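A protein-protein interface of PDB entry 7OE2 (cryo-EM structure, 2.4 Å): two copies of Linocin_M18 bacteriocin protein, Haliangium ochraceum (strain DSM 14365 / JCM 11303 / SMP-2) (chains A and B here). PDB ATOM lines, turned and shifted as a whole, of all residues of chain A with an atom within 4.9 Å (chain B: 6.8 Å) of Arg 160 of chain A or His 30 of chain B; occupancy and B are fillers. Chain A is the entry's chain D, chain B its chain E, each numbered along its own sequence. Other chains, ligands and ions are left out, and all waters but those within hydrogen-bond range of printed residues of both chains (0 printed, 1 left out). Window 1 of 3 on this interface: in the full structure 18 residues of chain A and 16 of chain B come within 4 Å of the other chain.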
ATOM      1  N   LEU A 153     -17.505  18.041   2.170  1.00  0.00           N
ATOM      2  CA  LEU A 153     -18.461  19.059   1.758  1.00  0.00           C
ATOM      3  C   LEU A 153     -19.806  18.429   1.452  1.00  0.00           C
ATOM      4  O   LEU A 153     -20.844  18.907   1.924  1.00  0.00           O
ATOM      5  CB  LEU A 153     -17.927  19.837   0.556  1.00  0.00           C
ATOM      6  CG  LEU A 153     -16.809  20.807   0.933  1.00  0.00           C
ATOM      7  CD1 LEU A 153     -15.872  21.055  -0.231  1.00  0.00           C
ATOM      8  CD2 LEU A 153     -17.366  22.106   1.483  1.00  0.00           C
ATOM      9  N   ALA A 156     -21.552  17.642   4.619  1.00  0.00           N
ATOM     10  CA  ALA A 156     -22.073  18.836   5.261  1.00  0.00           C
ATOM     11  C   ALA A 156     -23.366  19.263   4.596  1.00  0.00           C
ATOM     12  O   ALA A 156     -24.356  19.558   5.275  1.00  0.00           O
ATOM     13  CB  ALA A 156     -21.038  19.958   5.224  1.00  0.00           C
ATOM     14  N   ASP A 157     -23.402  19.202   3.264  1.00  0.00           N
ATOM     15  CA  ASP A 157     -24.612  19.574   2.557  1.00  0.00           C
ATOM     16  C   ASP A 157     -25.770  18.684   2.970  1.00  0.00           C
ATOM     17  O   ASP A 157     -26.865  19.177   3.259  1.00  0.00           O
ATOM     18  CB  ASP A 157     -24.379  19.511   1.051  1.00  0.00           C
ATOM     19  CG  ASP A 157     -25.474  20.186   0.273  1.00  0.00           C
ATOM     20  OD1 ASP A 157     -26.009  21.206   0.755  1.00  0.00           O
ATOM     21  OD2 ASP A 157     -25.809  19.694  -0.821  1.00  0.00           O
ATOM     22  N   THR A 158     -25.524  17.377   3.076  1.00  0.00           N
ATOM     23  CA  THR A 158     -26.582  16.481   3.517  1.00  0.00           C
ATOM     24  C   THR A 158     -27.084  16.898   4.889  1.00  0.00           C
ATOM     25  O   THR A 158     -28.292  17.056   5.097  1.00  0.00           O
ATOM     26  CB  THR A 158     -26.077  15.040   3.528  1.00  0.00           C
ATOM     27  OG1 THR A 158     -25.879  14.602   2.184  1.00  0.00           O
ATOM     28  CG2 THR A 158     -27.073  14.126   4.201  1.00  0.00           C
ATOM     29  N   LEU A 159     -26.162  17.180   5.810  1.00  0.00           N
ATOM     30  CA  LEU A 159     -26.589  17.565   7.143  1.00  0.00           C
ATOM     31  C   LEU A 159     -27.342  18.883   7.105  1.00  0.00           C
ATOM     32  O   LEU A 159     -28.280  19.084   7.878  1.00  0.00           O
ATOM     33  CB  LEU A 159     -25.391  17.634   8.089  1.00  0.00           C
ATOM     34  CG  LEU A 159     -24.706  16.296   8.390  1.00  0.00           C
ATOM     35  CD1 LEU A 159     -23.495  16.487   9.277  1.00  0.00           C
ATOM     36  CD2 LEU A 159     -25.674  15.299   9.010  1.00  0.00           C
ATOM     37  N   ARG A 160     -26.972  19.772   6.182  1.00  0.00           N
ATOM     38  CA  ARG A 160     -27.682  21.037   6.059  1.00  0.00           C
ATOM     39  C   ARG A 160     -29.105  20.827   5.564  1.00  0.00           C
ATOM     40  O   ARG A 160     -30.022  21.530   5.994  1.00  0.00           O
ATOM     41  CB  ARG A 160     -26.927  21.973   5.125  1.00  0.00           C
ATOM     42  CG  ARG A 160     -26.459  23.240   5.785  1.00  0.00           C
ATOM     43  CD  ARG A 160     -25.860  24.179   4.765  1.00  0.00           C
ATOM     44  NE  ARG A 160     -25.128  23.451   3.737  1.00  0.00           N
ATOM     45  CZ  ARG A 160     -23.817  23.253   3.751  1.00  0.00           C
ATOM     46  NH1 ARG A 160     -23.079  23.729   4.740  1.00  0.00           N
ATOM     47  NH2 ARG A 160     -23.246  22.580   2.769  1.00  0.00           N
ATOM     48  N   LYS A 161     -29.315  19.862   4.668  1.00  0.00           N
ATOM     49  CA  LYS A 161     -30.642  19.700   4.095  1.00  0.00           C
ATOM     50  C   LYS A 161     -31.603  19.005   5.041  1.00  0.00           C
ATOM     51  O   LYS A 161     -32.819  19.123   4.866  1.00  0.00           O
ATOM     52  CB  LYS A 161     -30.563  18.930   2.782  1.00  0.00           C
ATOM     53  CG  LYS A 161     -30.130  19.777   1.616  1.00  0.00           C
ATOM     54  CD  LYS A 161     -29.254  18.982   0.676  1.00  0.00           C
ATOM     55  CE  LYS A 161     -29.311  19.527  -0.732  1.00  0.00           C
ATOM     56  NZ  LYS A 161     -28.453  18.729  -1.649  1.00  0.00           N
ATOM     57  N   ALA A 162     -31.087  18.295   6.033  1.00  0.00           N
ATOM     58  CA  ALA A 162     -31.898  17.639   7.040  1.00  0.00           C
ATOM     59  C   ALA A 162     -32.191  18.549   8.219  1.00  0.00           C
ATOM     60  O   ALA A 162     -32.742  18.091   9.219  1.00  0.00           O
ATOM     61  CB  ALA A 162     -31.210  16.363   7.518  1.00  0.00           C
ATOM     62  N   GLY A 163     -31.823  19.819   8.126  1.00  0.00           N
ATOM     63  CA  GLY A 163     -32.045  20.756   9.196  1.00  0.00           C
ATOM     64  C   GLY A 163     -30.979  20.773  10.263  1.00  0.00           C
ATOM     65  O   GLY A 163     -31.079  21.577  11.197  1.00  0.00           O
ATOM     66  N   VAL A 164     -29.957  19.928  10.152  1.00  0.00           N
ATOM     67  CA  VAL A 164     -28.899  19.843  11.153  1.00  0.00           C
ATOM     68  C   VAL A 164     -27.853  20.891  10.799  1.00  0.00           C
ATOM     69  O   VAL A 164     -27.075  20.725   9.867  1.00  0.00           O
ATOM     70  CB  VAL A 164     -28.296  18.440  11.231  1.00  0.00           C
ATOM     71  CG1 VAL A 164     -27.381  18.332  12.434  1.00  0.00           C
ATOM     72  CG2 VAL A 164     -29.386  17.396  11.304  1.00  0.00           C
ATOM     73  N   THR A 165     -27.837  21.973  11.549  1.00  0.00           N
ATOM     74  CA  THR A 165     -26.836  23.013  11.382  1.00  0.00           C
ATOM     75  C   THR A 165     -25.649  22.727  12.295  1.00  0.00           C
ATOM     76  O   THR A 165     -25.459  21.607  12.773  1.00  0.00           O
ATOM     77  CB  THR A 165     -27.437  24.393  11.662  1.00  0.00           C
ATOM     78  OG1 THR A 165     -27.347  24.677  13.065  1.00  0.00           O
ATOM     79  CG2 THR A 165     -28.877  24.484  11.182  1.00  0.00           C
ATOM     80  N   TYR A 168     -19.280  21.366  11.895  1.00  0.00           N
ATOM     81  CA  TYR A 168     -19.203  19.948  11.591  1.00  0.00           C
ATOM     82  C   TYR A 168     -17.806  19.433  11.889  1.00  0.00           C
ATOM     83  O   TYR A 168     -16.815  20.050  11.497  1.00  0.00           O
ATOM     84  CB  TYR A 168     -19.577  19.688  10.134  1.00  0.00           C
ATOM     85  CG  TYR A 168     -20.971  20.140   9.804  1.00  0.00           C
ATOM     86  CD1 TYR A 168     -22.072  19.547  10.405  1.00  0.00           C
ATOM     87  CD2 TYR A 168     -21.193  21.177   8.914  1.00  0.00           C
ATOM     88  CE1 TYR A 168     -23.346  19.963  10.118  1.00  0.00           C
ATOM     89  CE2 TYR A 168     -22.465  21.599   8.618  1.00  0.00           C
ATOM     90  CZ  TYR A 168     -23.539  20.986   9.216  1.00  0.00           C
ATOM     91  OH  TYR A 168     -24.811  21.402   8.925  1.00  0.00           O
ATOM     92  N   GLU B  25     -31.804  28.666  15.517  1.00  0.00           N
ATOM     93  CA  GLU B  25     -30.548  28.125  15.006  1.00  0.00           C
ATOM     94  C   GLU B  25     -30.555  28.064  13.483  1.00  0.00           C
ATOM     95  O   GLU B  25     -29.566  28.429  12.837  1.00  0.00           O
ATOM     96  CB  GLU B  25     -30.240  26.757  15.632  1.00  0.00           C
ATOM     97  CG  GLU B  25     -31.395  25.770  15.755  1.00  0.00           C
ATOM     98  CD  GLU B  25     -31.495  24.784  14.604  1.00  0.00           C
ATOM     99  OE1 GLU B  25     -30.579  24.762  13.768  1.00  0.00           O
ATOM    100  OE2 GLU B  25     -32.481  24.021  14.542  1.00  0.00           O
ATOM    101  N   ILE B  26     -31.682  27.666  12.892  1.00  0.00           N
ATOM    102  CA  ILE B  26     -31.811  27.664  11.438  1.00  0.00           C
ATOM    103  C   ILE B  26     -31.667  29.072  10.876  1.00  0.00           C
ATOM    104  O   ILE B  26     -30.974  29.289   9.877  1.00  0.00           O
ATOM    105  CB  ILE B  26     -33.148  27.027  11.024  1.00  0.00           C
ATOM    106  CG1 ILE B  26     -33.177  25.556  11.435  1.00  0.00           C
ATOM    107  CG2 ILE B  26     -33.422  27.255   9.532  1.00  0.00           C
ATOM    108  CD1 ILE B  26     -33.630  24.618  10.378  1.00  0.00           C
ATOM    109  N   PHE B  27     -32.325  30.051  11.497  1.00  0.00           N
ATOM    110  CA  PHE B  27     -32.272  31.405  10.958  1.00  0.00           C
ATOM    111  C   PHE B  27     -30.869  31.988  11.051  1.00  0.00           C
ATOM    112  O   PHE B  27     -30.378  32.585  10.090  1.00  0.00           O
ATOM    113  CB  PHE B  27     -33.282  32.304  11.667  1.00  0.00           C
ATOM    114  CG  PHE B  27     -34.698  32.018  11.298  1.00  0.00           C
ATOM    115  CD1 PHE B  27     -35.033  31.721   9.994  1.00  0.00           C
ATOM    116  CD2 PHE B  27     -35.692  32.024  12.252  1.00  0.00           C
ATOM    117  CE1 PHE B  27     -36.328  31.449   9.652  1.00  0.00           C
ATOM    118  CE2 PHE B  27     -36.984  31.744  11.909  1.00  0.00           C
ATOM    119  CZ  PHE B  27     -37.304  31.460  10.614  1.00  0.00           C
ATOM    120  N   GLN B  28     -30.203  31.817  12.193  1.00  0.00           N
ATOM    121  CA  GLN B  28     -28.855  32.343  12.330  1.00  0.00           C
ATOM    122  C   GLN B  28     -27.872  31.624  11.420  1.00  0.00           C
ATOM    123  O   GLN B  28     -26.887  32.224  10.983  1.00  0.00           O
ATOM    124  CB  GLN B  28     -28.397  32.262  13.781  1.00  0.00           C
ATOM    125  CG  GLN B  28     -28.862  33.430  14.607  1.00  0.00           C
ATOM    126  CD  GLN B  28     -28.939  33.117  16.076  1.00  0.00           C
ATOM    127  OE1 GLN B  28     -29.022  31.960  16.475  1.00  0.00           O
ATOM    128  NE2 GLN B  28     -28.925  34.156  16.896  1.00  0.00           N
ATOM    129  N   GLY B  29     -28.118  30.357  11.109  1.00  0.00           N
ATOM    130  CA  GLY B  29     -27.228  29.663  10.210  1.00  0.00           C
ATOM    131  C   GLY B  29     -27.431  29.914   8.730  1.00  0.00           C
ATOM    132  O   GLY B  29     -26.454  29.935   7.980  1.00  0.00           O
ATOM    133  N   HIS B  30     -28.671  30.109   8.287  1.00  0.00           N
ATOM    134  CA  HIS B  30     -28.992  29.985   6.874  1.00  0.00           C
ATOM    135  C   HIS B  30     -29.434  31.272   6.194  1.00  0.00           C
ATOM    136  O   HIS B  30     -29.599  31.268   4.973  1.00  0.00           O
ATOM    137  CB  HIS B  30     -30.086  28.926   6.675  1.00  0.00           C
ATOM    138  CG  HIS B  30     -29.675  27.547   7.082  1.00  0.00           C
ATOM    139  ND1 HIS B  30     -28.403  27.247   7.512  1.00  0.00           N
ATOM    140  CD2 HIS B  30     -30.368  26.387   7.120  1.00  0.00           C
ATOM    141  CE1 HIS B  30     -28.330  25.962   7.800  1.00  0.00           C
ATOM    142  NE2 HIS B  30     -29.509  25.416   7.568  1.00  0.00           N
ATOM    143  N   LEU B  31     -29.633  32.364   6.924  1.00  0.00           N
ATOM    144  CA  LEU B  31     -30.081  33.615   6.311  1.00  0.00           C
ATOM    145  C   LEU B  31     -28.884  34.322   5.687  1.00  0.00           C
ATOM    146  O   LEU B  31     -28.107  34.979   6.377  1.00  0.00           O
ATOM    147  CB  LEU B  31     -30.769  34.504   7.338  1.00  0.00           C
ATOM    148  CG  LEU B  31     -32.237  34.208   7.637  1.00  0.00           C
ATOM    149  CD1 LEU B  31     -32.662  34.960   8.868  1.00  0.00           C
ATOM    150  CD2 LEU B  31     -33.117  34.545   6.454  1.00  0.00           C
ATOM    151  N   ALA B  32     -28.743  34.206   4.370  1.00  0.00           N
ATOM    152  CA  ALA B  32     -27.558  34.733   3.703  1.00  0.00           C
ATOM    153  C   ALA B  32     -27.713  36.202   3.327  1.00  0.00           C
ATOM    154  O   ALA B  32     -26.763  36.976   3.459  1.00  0.00           O
ATOM    155  CB  ALA B  32     -27.242  33.894   2.469  1.00  0.00           C
ATOM    156  N   GLY B  33     -28.898  36.605   2.863  1.00  0.00           N
ATOM    157  CA  GLY B  33     -29.101  37.990   2.470  1.00  0.00           C
ATOM    158  C   GLY B  33     -28.860  38.974   3.600  1.00  0.00           C
ATOM    159  O   GLY B  33     -28.296  40.046   3.388  1.00  0.00           O
ATOM    160  N   LYS B  35     -26.741  38.764   5.877  1.00  0.00           N
ATOM    161  CA  LYS B  35     -25.312  38.934   6.084  1.00  0.00           C
ATOM    162  C   LYS B  35     -24.696  39.958   5.142  1.00  0.00           C
ATOM    163  O   LYS B  35     -23.609  40.459   5.425  1.00  0.00           O
ATOM    164  CB  LYS B  35     -24.587  37.599   5.913  1.00  0.00           C
ATOM    165  CG  LYS B  35     -24.668  36.678   7.102  1.00  0.00           C
ATOM    166  CD  LYS B  35     -24.774  35.234   6.663  1.00  0.00           C
ATOM    167  CE  LYS B  35     -24.662  34.294   7.849  1.00  0.00           C
ATOM    168  NZ  LYS B  35     -25.564  33.118   7.721  1.00  0.00           N
ATOM    169  N   ALA B 108     -39.081  26.967   9.044  1.00  0.00           N
ATOM    170  CA  ALA B 108     -38.003  27.943   9.123  1.00  0.00           C
ATOM    171  C   ALA B 108     -37.164  27.956   7.850  1.00  0.00           C
ATOM    172  O   ALA B 108     -36.802  29.030   7.360  1.00  0.00           O
ATOM    173  CB  ALA B 108     -37.131  27.677  10.346  1.00  0.00           C
ATOM    174  N   GLU B 109     -36.856  26.783   7.285  1.00  0.00           N
ATOM    175  CA  GLU B 109     -36.110  26.769   6.032  1.00  0.00           C
ATOM    176  C   GLU B 109     -36.945  27.303   4.879  1.00  0.00           C
ATOM    177  O   GLU B 109     -36.401  27.941   3.976  1.00  0.00           O
ATOM    178  CB  GLU B 109     -35.569  25.368   5.711  1.00  0.00           C
ATOM    179  CG  GLU B 109     -36.589  24.257   5.497  1.00  0.00           C
ATOM    180  CD  GLU B 109     -37.200  24.216   4.095  1.00  0.00           C
ATOM    181  OE1 GLU B 109     -38.334  23.707   3.957  1.00  0.00           O
ATOM    182  OE2 GLU B 109     -36.553  24.691   3.136  1.00  0.00           O
ATOM    183  N   VAL B 112     -36.702  31.047   5.246  1.00  0.00           N
ATOM    184  CA  VAL B 112     -35.372  31.451   4.800  1.00  0.00           C
ATOM    185  C   VAL B 112     -35.319  31.481   3.283  1.00  0.00           C
ATOM    186  O   VAL B 112     -34.782  32.418   2.682  1.00  0.00           O
ATOM    187  CB  VAL B 112     -34.297  30.511   5.380  1.00  0.00           C
ATOM    188  CG1 VAL B 112     -33.028  30.564   4.542  1.00  0.00           C
ATOM    189  CG2 VAL B 112     -33.988  30.867   6.806  1.00  0.00           C
ATOM    190  N   GLU B 113     -35.875  30.455   2.644  1.00  0.00           N
ATOM    191  CA  GLU B 113     -35.897  30.407   1.191  1.00  0.00           C
ATOM    192  C   GLU B 113     -36.666  31.584   0.615  1.00  0.00           C
ATOM    193  O   GLU B 113     -36.213  32.212  -0.342  1.00  0.00           O
ATOM    194  CB  GLU B 113     -36.495  29.082   0.727  1.00  0.00           C
ATOM    195  CG  GLU B 113     -36.871  29.050  -0.731  1.00  0.00           C
ATOM    196  CD  GLU B 113     -37.660  27.814  -1.103  1.00  0.00           C
ATOM    197  OE1 GLU B 113     -38.075  27.703  -2.274  1.00  0.00           O
ATOM    198  OE2 GLU B 113     -37.868  26.949  -0.228  1.00  0.00           O
ATOM    199  N   ASP B 116     -34.516  34.917   1.189  1.00  0.00           N
ATOM    200  CA  ASP B 116     -33.273  34.961   0.432  1.00  0.00           C
ATOM    201  C   ASP B 116     -33.518  34.936  -1.064  1.00  0.00           C
ATOM    202  O   ASP B 116     -32.776  35.571  -1.817  1.00  0.00           O
ATOM    203  CB  ASP B 116     -32.360  33.812   0.847  1.00  0.00           C
ATOM    204  CG  ASP B 116     -31.415  34.205   1.953  1.00  0.00           C
ATOM    205  OD1 ASP B 116     -31.197  35.416   2.138  1.00  0.00           O
ATOM    206  OD2 ASP B 116     -30.895  33.314   2.650  1.00  0.00           O
ATOM    207  N   PRO B 174     -24.826  27.138  -3.763  1.00  0.00           N
ATOM    208  CA  PRO B 174     -24.350  25.867  -3.178  1.00  0.00           C
ATOM    209  C   PRO B 174     -23.369  25.103  -4.054  1.00  0.00           C
ATOM    210  O   PRO B 174     -22.323  24.657  -3.564  1.00  0.00           O
ATOM    211  CB  PRO B 174     -25.653  25.087  -2.947  1.00  0.00           C
ATOM    212  CG  PRO B 174     -26.677  25.767  -3.757  1.00  0.00           C
ATOM    213  CD  PRO B 174     -26.288  27.186  -3.888  1.00  0.00           C
ATOM    214  N   TYR B 177     -20.068  26.980  -4.322  1.00  0.00           N
ATOM    215  CA  TYR B 177     -19.358  26.900  -3.052  1.00  0.00           C
ATOM    216  C   TYR B 177     -18.670  25.552  -2.886  1.00  0.00           C
ATOM    217  O   TYR B 177     -17.487  25.484  -2.528  1.00  0.00           O
ATOM    218  CB  TYR B 177     -20.323  27.153  -1.893  1.00  0.00           C
ATOM    219  CG  TYR B 177     -19.636  27.248  -0.558  1.00  0.00           C
ATOM    220  CD1 TYR B 177     -19.318  26.108   0.163  1.00  0.00           C
ATOM    221  CD2 TYR B 177     -19.295  28.475  -0.026  1.00  0.00           C
ATOM    222  CE1 TYR B 177     -18.679  26.189   1.366  1.00  0.00           C
ATOM    223  CE2 TYR B 177     -18.665  28.569   1.179  1.00  0.00           C
ATOM    224  CZ  TYR B 177     -18.356  27.424   1.873  1.00  0.00           C
ATOM    225  OH  TYR B 177     -17.722  27.520   3.081  1.00  0.00           O
ATOM    226  N   ASP B 178     -19.399  24.465  -3.127  1.00  0.00           N
ATOM    227  CA  ASP B 178     -18.824  23.145  -2.910  1.00  0.00           C
ATOM    228  C   ASP B 178     -17.688  22.870  -3.886  1.00  0.00           C
ATOM    229  O   ASP B 178     -16.632  22.355  -3.492  1.00  0.00           O
ATOM    230  CB  ASP B 178     -19.912  22.079  -3.005  1.00  0.00           C
ATOM    231  CG  ASP B 178     -20.858  22.113  -1.820  1.00  0.00           C
ATOM    232  OD1 ASP B 178     -20.441  22.565  -0.735  1.00  0.00           O
ATOM    233  OD2 ASP B 178     -22.025  21.699  -1.970  1.00  0.00           O
ATOM    234  N   ARG B 205     -21.986  31.379   1.741  1.00  0.00           N
ATOM    235  CA  ARG B 205     -22.708  30.369   0.992  1.00  0.00           C
ATOM    236  C   ARG B 205     -24.190  30.716   1.059  1.00  0.00           C
ATOM    237  O   ARG B 205     -24.779  30.721   2.142  1.00  0.00           O
ATOM    238  CB  ARG B 205     -22.432  28.984   1.576  1.00  0.00           C
ATOM    239  CG  ARG B 205     -22.994  27.821   0.807  1.00  0.00           C
ATOM    240  CD  ARG B 205     -22.908  26.549   1.638  1.00  0.00           C
ATOM    241  NE  ARG B 205     -23.011  25.345   0.826  1.00  0.00           N
ATOM    242  CZ  ARG B 205     -24.158  24.763   0.502  1.00  0.00           C
ATOM    243  NH1 ARG B 205     -25.303  25.272   0.927  1.00  0.00           N
ATOM    244  NH2 ARG B 205     -24.159  23.674  -0.245  1.00  0.00           N
ATOM    245  N   ALA B 206     -24.778  31.031  -0.084  1.00  0.00           N
ATOM    246  CA  ALA B 206     -26.179  31.413  -0.185  1.00  0.00           C
ATOM    247  C   ALA B 206     -26.928  30.300  -0.903  1.00  0.00           C
ATOM    248  O   ALA B 206     -26.731  30.086  -2.101  1.00  0.00           O
ATOM    249  CB  ALA B 206     -26.332  32.743  -0.916  1.00  0.00           C
ATOM    250  N   ASN B 207     -27.795  29.606  -0.167  1.00  0.00           N
ATOM    251  CA  ASN B 207     -28.510  28.462  -0.722  1.00  0.00           C
ATOM    252  C   ASN B 207     -29.482  28.868  -1.822  1.00  0.00           C
ATOM    253  O   ASN B 207     -29.722  28.089  -2.748  1.00  0.00           O
ATOM    254  CB  ASN B 207     -29.238  27.722   0.401  1.00  0.00           C
ATOM    255  CG  ASN B 207     -29.938  26.470  -0.080  1.00  0.00           C
ATOM    256  OD1 ASN B 207     -29.300  25.482  -0.428  1.00  0.00           O
ATOM    257  ND2 ASN B 207     -31.262  26.506  -0.096  1.00  0.00           N
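The side-chain carboxylate of Asp 157 of chain A lies within salt-bridge range of the guanidinium group of Arg 160 of chain A (3.7 Å).
OD2 of Asp 157 of chain A lies within salt-bridge range of NZ of Lys 161 of chain A, 2.9 Å away.
The side-chain carboxylate of Asp 178 of chain B lies within salt-bridge range of the guanidinium group of Arg 205 of chain B (3.4 Å).
Among the printed residues, merely in contact across the chains: Leu 153 of chain A with Asp 178 of chain B (3.6 Å), Thr 165 of chain A with His 30 of chain B (3.7 Å) and Arg 160 of chain A with His 30 of chain B (3.9 Å).
No position is printed for both chains.
Of the 6 pairs that touch across the chains among the printed residues, none has its exchanged pair printed and touching as well.
The guanidinium group (NH2) of Arg 205 of chain B is in salt-bridge range of the side-chain carboxylate (OD1) of Asp 157 of chain A, at 3.2 Å.
The side-chain hydroxyl of Thr 165 of chain A sits close to the side-chain carboxylate of Glu 25 of chain B (3.3 Å).
The guanidinium group (NH2) of Arg 160 of chain A lies close to the guanidinium group (NH2) of Arg 205 of chain B, at 3.3 Å.
Of the printed residues of chain B, Asp 157 of chain A touches Arg 205 (3.2 Å).
Arg 160 of chain A touches just these residues of chain B: His 30 and Arg 205.
Of the printed residues of chain A, Glu 25 of chain B touches Thr 165 (3.1 Å).
Of chain A, only Arg 160 and Thr 165 come within 4 Å of His 30 of chain B.
Printed residues of chain A within 4 Å of Arg 205 of chain B: Asp 157 and Arg 160.
The nearest residue of chain B that does not touch Arg 160 of chain A is Asp 178 of chain B (4.5 Å).
The nearest printed residue of chain A that does not touch His 30 of chain B is Gly 163 of chain A (5.5 Å).
The nearest printed residue of chain B that does not touch Thr 165 of chain A is Ile 26 of chain B (4.3 Å).
Hydrophobic or aromatic side chains of chain A that line the printed part of chain B: Leu 153.
Hydrophobic or aromatic side chains of chain B that line the printed part of chain A: His 30.
Along chain B the printed residues that touch a printed residue of chain A span positions 25 to 205.
Among the printed residues, 6 pairs touch across the chains.
Among the printed residues, Asp or Glu carboxylates within 4 Å of a Lys or Arg side-chain nitrogen of the other chain: Asp 157 of chain A with Arg 205 of chain B (3.2 Å).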
